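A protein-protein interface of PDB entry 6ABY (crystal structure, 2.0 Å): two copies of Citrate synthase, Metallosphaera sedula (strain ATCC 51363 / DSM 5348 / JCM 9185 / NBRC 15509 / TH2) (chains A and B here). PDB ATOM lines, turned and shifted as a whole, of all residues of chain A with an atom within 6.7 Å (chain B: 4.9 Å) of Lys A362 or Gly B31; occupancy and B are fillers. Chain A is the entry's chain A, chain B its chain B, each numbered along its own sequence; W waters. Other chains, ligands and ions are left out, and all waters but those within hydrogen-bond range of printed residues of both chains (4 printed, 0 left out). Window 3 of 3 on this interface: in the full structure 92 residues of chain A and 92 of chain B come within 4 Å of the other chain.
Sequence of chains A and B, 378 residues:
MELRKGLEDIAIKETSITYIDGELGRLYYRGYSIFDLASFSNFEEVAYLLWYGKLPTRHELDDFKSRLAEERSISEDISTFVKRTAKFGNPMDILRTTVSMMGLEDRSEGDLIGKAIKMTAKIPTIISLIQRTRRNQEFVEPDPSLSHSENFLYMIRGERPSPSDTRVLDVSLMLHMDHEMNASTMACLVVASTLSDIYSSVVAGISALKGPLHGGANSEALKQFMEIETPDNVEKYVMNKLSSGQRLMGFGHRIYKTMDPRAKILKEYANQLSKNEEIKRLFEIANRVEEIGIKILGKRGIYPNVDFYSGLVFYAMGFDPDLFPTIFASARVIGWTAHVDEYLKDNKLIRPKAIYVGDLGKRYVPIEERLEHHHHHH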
ATOM      1  N   TYR A 356       1.201  12.411  -3.684  1.00  0.00           N
ATOM      2  CA  TYR A 356       2.114  13.242  -2.882  1.00  0.00           C
ATOM      3  C   TYR A 356       1.325  14.395  -2.247  1.00  0.00           C
ATOM      4  O   TYR A 356       0.594  15.038  -2.975  1.00  0.00           O
ATOM      5  CB  TYR A 356       3.269  13.761  -3.737  1.00  0.00           C
ATOM      6  CG  TYR A 356       4.290  14.442  -2.878  1.00  0.00           C
ATOM      7  CD1 TYR A 356       5.099  13.706  -2.039  1.00  0.00           C
ATOM      8  CD2 TYR A 356       4.426  15.826  -2.870  1.00  0.00           C
ATOM      9  CE1 TYR A 356       6.070  14.318  -1.259  1.00  0.00           C
ATOM     10  CE2 TYR A 356       5.339  16.439  -2.031  1.00  0.00           C
ATOM     11  CZ  TYR A 356       6.180  15.688  -1.235  1.00  0.00           C
ATOM     12  OH  TYR A 356       7.119  16.302  -0.447  1.00  0.00           O
ATOM     13  N   GLY A 358       2.939  16.480   0.443  1.00  0.00           N
ATOM     14  CA  GLY A 358       3.918  17.207   1.271  1.00  0.00           C
ATOM     15  C   GLY A 358       4.346  18.499   0.604  1.00  0.00           C
ATOM     16  O   GLY A 358       3.648  18.987  -0.339  1.00  0.00           O
ATOM     17  N   ASP A 359       5.524  18.983   0.994  1.00  0.00           N
ATOM     18  CA  ASP A 359       6.107  20.224   0.439  1.00  0.00           C
ATOM     19  C   ASP A 359       7.153  19.904  -0.605  1.00  0.00           C
ATOM     20  O   ASP A 359       7.589  18.729  -0.702  1.00  0.00           O
ATOM     21  CB  ASP A 359       6.702  21.115   1.510  1.00  0.00           C
ATOM     22  CG  ASP A 359       5.623  21.572   2.459  1.00  0.00           C
ATOM     23  OD1 ASP A 359       4.615  22.172   1.984  1.00  0.00           O
ATOM     24  OD2 ASP A 359       5.763  21.243   3.625  1.00  0.00           O
ATOM     25  N   LEU A 360       7.464  20.936  -1.371  1.00  0.00           N
ATOM     26  CA  LEU A 360       8.446  20.942  -2.474  1.00  0.00           C
ATOM     27  C   LEU A 360       9.305  22.202  -2.388  1.00  0.00           C
ATOM     28  O   LEU A 360       8.797  23.241  -1.903  1.00  0.00           O
ATOM     29  CB  LEU A 360       7.661  20.899  -3.788  1.00  0.00           C
ATOM     30  CG  LEU A 360       6.924  19.599  -4.053  1.00  0.00           C
ATOM     31  CD1 LEU A 360       6.002  19.704  -5.252  1.00  0.00           C
ATOM     32  CD2 LEU A 360       7.916  18.471  -4.241  1.00  0.00           C
ATOM     33  N   GLY A 361      10.546  22.094  -2.856  1.00  0.00           N
ATOM     34  CA  GLY A 361      11.455  23.211  -3.101  1.00  0.00           C
ATOM     35  C   GLY A 361      11.927  23.826  -1.796  1.00  0.00           C
ATOM     36  O   GLY A 361      12.254  24.982  -1.809  1.00  0.00           O
ATOM     37  N   LYS A 362      11.928  23.092  -0.698  1.00  0.00           N
ATOM     38  CA  LYS A 362      12.441  23.620   0.596  1.00  0.00           C
ATOM     39  C   LYS A 362      13.929  23.972   0.488  1.00  0.00           C
ATOM     40  O   LYS A 362      14.713  23.305  -0.223  1.00  0.00           O
ATOM     41  CB  LYS A 362      12.204  22.616   1.713  1.00  0.00           C
ATOM     42  CG  LYS A 362      10.759  22.391   2.071  1.00  0.00           C
ATOM     43  CD  LYS A 362      10.545  21.512   3.266  1.00  0.00           C
ATOM     44  CE  LYS A 362      11.317  21.973   4.475  1.00  0.00           C
ATOM     45  NZ  LYS A 362      10.524  22.934   5.253  1.00  0.00           N
ATOM     46  N   ARG A 363      14.328  25.037   1.161  1.00  0.00           N
ATOM     47  CA  ARG A 363      15.695  25.571   1.057  1.00  0.00           C
ATOM     48  C   ARG A 363      16.542  24.883   2.118  1.00  0.00           C
ATOM     49  O   ARG A 363      16.201  24.942   3.304  1.00  0.00           O
ATOM     50  CB  ARG A 363      15.714  27.094   1.236  1.00  0.00           C
ATOM     51  CG  ARG A 363      17.000  27.733   0.746  1.00  0.00           C
ATOM     52  CD  ARG A 363      17.009  29.228   1.014  1.00  0.00           C
ATOM     53  NE  ARG A 363      17.860  29.537   2.160  1.00  0.00           N
ATOM     54  CZ  ARG A 363      17.439  29.879   3.374  1.00  0.00           C
ATOM     55  NH1 ARG A 363      16.148  29.987   3.639  1.00  0.00           N
ATOM     56  NH2 ARG A 363      18.324  30.119   4.329  1.00  0.00           N
ATOM     57  N   TYR A 364      17.630  24.263   1.696  1.00  0.00           N
ATOM     58  CA  TYR A 364      18.515  23.533   2.616  1.00  0.00           C
ATOM     59  C   TYR A 364      19.262  24.580   3.431  1.00  0.00           C
ATOM     60  O   TYR A 364      19.893  25.479   2.877  1.00  0.00           O
ATOM     61  CB  TYR A 364      19.496  22.625   1.877  1.00  0.00           C
ATOM     62  CG  TYR A 364      20.365  21.879   2.847  1.00  0.00           C
ATOM     63  CD1 TYR A 364      21.530  22.453   3.319  1.00  0.00           C
ATOM     64  CD2 TYR A 364      19.980  20.647   3.357  1.00  0.00           C
ATOM     65  CE1 TYR A 364      22.345  21.804   4.238  1.00  0.00           C
ATOM     66  CE2 TYR A 364      20.773  19.987   4.274  1.00  0.00           C
ATOM     67  CZ  TYR A 364      21.969  20.556   4.709  1.00  0.00           C
ATOM     68  OH  TYR A 364      22.767  19.916   5.627  1.00  0.00           O
ATOM     69  N   TYR B  28      12.752  14.644  -4.504  1.00  0.00           N
ATOM     70  CA  TYR B  28      12.732  15.367  -3.222  1.00  0.00           C
ATOM     71  C   TYR B  28      12.485  14.365  -2.111  1.00  0.00           C
ATOM     72  O   TYR B  28      11.581  13.534  -2.221  1.00  0.00           O
ATOM     73  CB  TYR B  28      11.665  16.472  -3.209  1.00  0.00           C
ATOM     74  CG  TYR B  28      11.840  17.518  -4.263  1.00  0.00           C
ATOM     75  CD1 TYR B  28      12.426  18.734  -3.992  1.00  0.00           C
ATOM     76  CD2 TYR B  28      11.409  17.268  -5.558  1.00  0.00           C
ATOM     77  CE1 TYR B  28      12.630  19.653  -5.008  1.00  0.00           C
ATOM     78  CE2 TYR B  28      11.568  18.187  -6.568  1.00  0.00           C
ATOM     79  CZ  TYR B  28      12.164  19.391  -6.283  1.00  0.00           C
ATOM     80  OH  TYR B  28      12.337  20.253  -7.312  1.00  0.00           O
ATOM     81  N   TYR B  29      13.235  14.541  -1.023  1.00  0.00           N
ATOM     82  CA  TYR B  29      13.031  13.899   0.299  1.00  0.00           C
ATOM     83  C   TYR B  29      12.503  14.955   1.273  1.00  0.00           C
ATOM     84  O   TYR B  29      13.220  15.926   1.580  1.00  0.00           O
ATOM     85  CB  TYR B  29      14.360  13.332   0.837  1.00  0.00           C
ATOM     86  CG  TYR B  29      14.990  12.173   0.097  1.00  0.00           C
ATOM     87  CD1 TYR B  29      14.333  11.397  -0.851  1.00  0.00           C
ATOM     88  CD2 TYR B  29      16.259  11.746   0.475  1.00  0.00           C
ATOM     89  CE1 TYR B  29      14.953  10.299  -1.464  1.00  0.00           C
ATOM     90  CE2 TYR B  29      16.891  10.677  -0.138  1.00  0.00           C
ATOM     91  CZ  TYR B  29      16.252   9.952  -1.122  1.00  0.00           C
ATOM     92  OH  TYR B  29      16.902   8.863  -1.646  1.00  0.00           O
ATOM     93  N   ARG B  30      11.268  14.783   1.752  1.00  0.00           N
ATOM     94  CA  ARG B  30      10.607  15.700   2.696  1.00  0.00           C
ATOM     95  C   ARG B  30      10.696  17.143   2.182  1.00  0.00           C
ATOM     96  O   ARG B  30      10.918  18.025   2.979  1.00  0.00           O
ATOM     97  CB  ARG B  30      11.260  15.589   4.073  1.00  0.00           C
ATOM     98  CG  ARG B  30      11.158  14.204   4.682  1.00  0.00           C
ATOM     99  CD  ARG B  30       9.825  13.913   5.298  1.00  0.00           C
ATOM    100  NE  ARG B  30       9.750  12.687   6.107  1.00  0.00           N
ATOM    101  CZ  ARG B  30       8.596  12.102   6.418  1.00  0.00           C
ATOM    102  NH1 ARG B  30       7.461  12.683   6.056  1.00  0.00           N
ATOM    103  NH2 ARG B  30       8.555  10.971   7.102  1.00  0.00           N
ATOM    104  N   GLY B  31      10.578  17.362   0.886  1.00  0.00           N
ATOM    105  CA  GLY B  31      10.599  18.710   0.289  1.00  0.00           C
ATOM    106  C   GLY B  31      11.977  19.201  -0.104  1.00  0.00           C
ATOM    107  O   GLY B  31      12.052  20.225  -0.795  1.00  0.00           O
ATOM    108  N   TYR B  32      13.057  18.519   0.295  1.00  0.00           N
ATOM    109  CA  TYR B  32      14.420  18.959  -0.030  1.00  0.00           C
ATOM    110  C   TYR B  32      14.873  18.261  -1.310  1.00  0.00           C
ATOM    111  O   TYR B  32      14.772  17.006  -1.472  1.00  0.00           O
ATOM    112  CB  TYR B  32      15.376  18.735   1.134  1.00  0.00           C
ATOM    113  CG  TYR B  32      15.058  19.542   2.349  1.00  0.00           C
ATOM    114  CD1 TYR B  32      15.532  20.840   2.473  1.00  0.00           C
ATOM    115  CD2 TYR B  32      14.272  19.032   3.349  1.00  0.00           C
ATOM    116  CE1 TYR B  32      15.245  21.605   3.588  1.00  0.00           C
ATOM    117  CE2 TYR B  32      14.033  19.754   4.507  1.00  0.00           C
ATOM    118  CZ  TYR B  32      14.492  21.059   4.605  1.00  0.00           C
ATOM    119  OH  TYR B  32      14.188  21.798   5.703  1.00  0.00           O
ATOM    120  N   SER B  33      15.485  19.039  -2.180  1.00  0.00           N
ATOM    121  CA  SER B  33      16.035  18.534  -3.457  1.00  0.00           C
ATOM    122  C   SER B  33      17.152  17.514  -3.170  1.00  0.00           C
ATOM    123  O   SER B  33      18.081  17.793  -2.337  1.00  0.00           O
ATOM    124  CB  SER B  33      16.559  19.652  -4.316  1.00  0.00           C
ATOM    125  OG  SER B  33      17.240  19.132  -5.460  1.00  0.00           O
ATOM    126  N   ASP B  36      20.608  19.139  -3.432  1.00  0.00           N
ATOM    127  CA  ASP B  36      21.062  19.865  -2.204  1.00  0.00           C
ATOM    128  C   ASP B  36      21.537  18.875  -1.140  1.00  0.00           C
ATOM    129  O   ASP B  36      22.557  19.154  -0.465  1.00  0.00           O
ATOM    130  CB  ASP B  36      19.958  20.809  -1.691  1.00  0.00           C
ATOM    131  CG  ASP B  36      19.722  22.014  -2.605  1.00  0.00           C
ATOM    132  OD1 ASP B  36      20.626  22.319  -3.428  1.00  0.00           O
ATOM    133  OD2 ASP B  36      18.584  22.578  -2.568  1.00  0.00           O
HETATM  134  O   HOH W   1       9.617  15.272  -0.972  1.00  0.00           O
HETATM  135  O   HOH W   2      16.017  23.801   5.779  1.00  0.00           O
HETATM  136  O   HOH W   3      18.490  24.861  -0.961  1.00  0.00           O
HETATM  137  O   HOH W   4      16.679  21.602  -0.915  1.00  0.00           O
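No position is printed for both chains.
Of the 11 pairs that touch across the chains among the printed residues, none has its exchanged pair printed and touching as well.
N of Lys A362 lies within hydrogen-bond range of O of Gly B31.
O of Gly B31 is in hydrogen-bond range of N of Gly A361 (3.2 Å).
Of chain B, only Arg B30 (3.5 Å), Gly B31 (2.9 Å) and Tyr B32 (3.1 Å) come within 4 Å of Lys A362.
Gly B31 touches five residues of chain A.
Printed residues of chain A within 4 Å of Tyr B32: Lys A362 (3.1 Å), Arg A363 (3.5 Å) and Tyr A364 (3.9 Å).
Printed residues of chain B within 4 Å of Arg A363: Tyr B32.
Of the printed residues of chain B, Tyr A356 touches Gly B31.
Printed residues of chain A within 4 Å of Arg B30: Lys A362 (3.5 Å).
Gly A358 touches none of the printed residues of chain B.
The nearest printed residue of chain B that does not touch Gly A361 is Tyr B32 (5.4 Å).
Water W4 lies within hydrogen-bond range of O of Lys A362, OD2 of Asp B36 and N of Ser B33.
Water W2 lies within hydrogen-bond range of OH of Tyr B32 and O of Arg A363.
Water W1 lies within hydrogen-bond range of OH of Tyr A356 (2.8 Å), O of Tyr B28 (2.9 Å), N of Gly B31 (3.0 Å) and N of Arg B30 (3.2 Å).
Water W3 bridges the side-chain carboxylate of Asp B36 (2.8 Å) and the backbone NH of Tyr A364 (2.9 Å).
The side-chain hydroxyl of Tyr A356 is in hydrogen-bond range of the backbone carbonyl oxygen of Asp A359.
Tyr A356 touches Gly B31 (OH to N, 3.9 Å).
Gly B31 touches Asp A359.
Leu A360 touches Tyr B28.
Leu A360 touches Gly B31 (C to O, 3.7 Å).
N of Gly A361 touches CE1 of Tyr B28, at 3.9 Å.
Lys A362 touches Arg B30 (CD to O, 3.5 Å).
Tyr B32 touches Lys A362 (OH to CE, 3.1 Å).
CE1 of Tyr B32 touches O of Arg A363, at 3.5 Å.
Tyr B32 touches Tyr A364.
Hydrophobic or aromatic side chains of chain B within 4 Å of the printed part of chain A: Tyr B28 and Tyr B32.
Of the 8 printed residues of chain A, 7 touch a printed residue of chain B.
Among the printed residues, 11 pairs touch across the chains.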
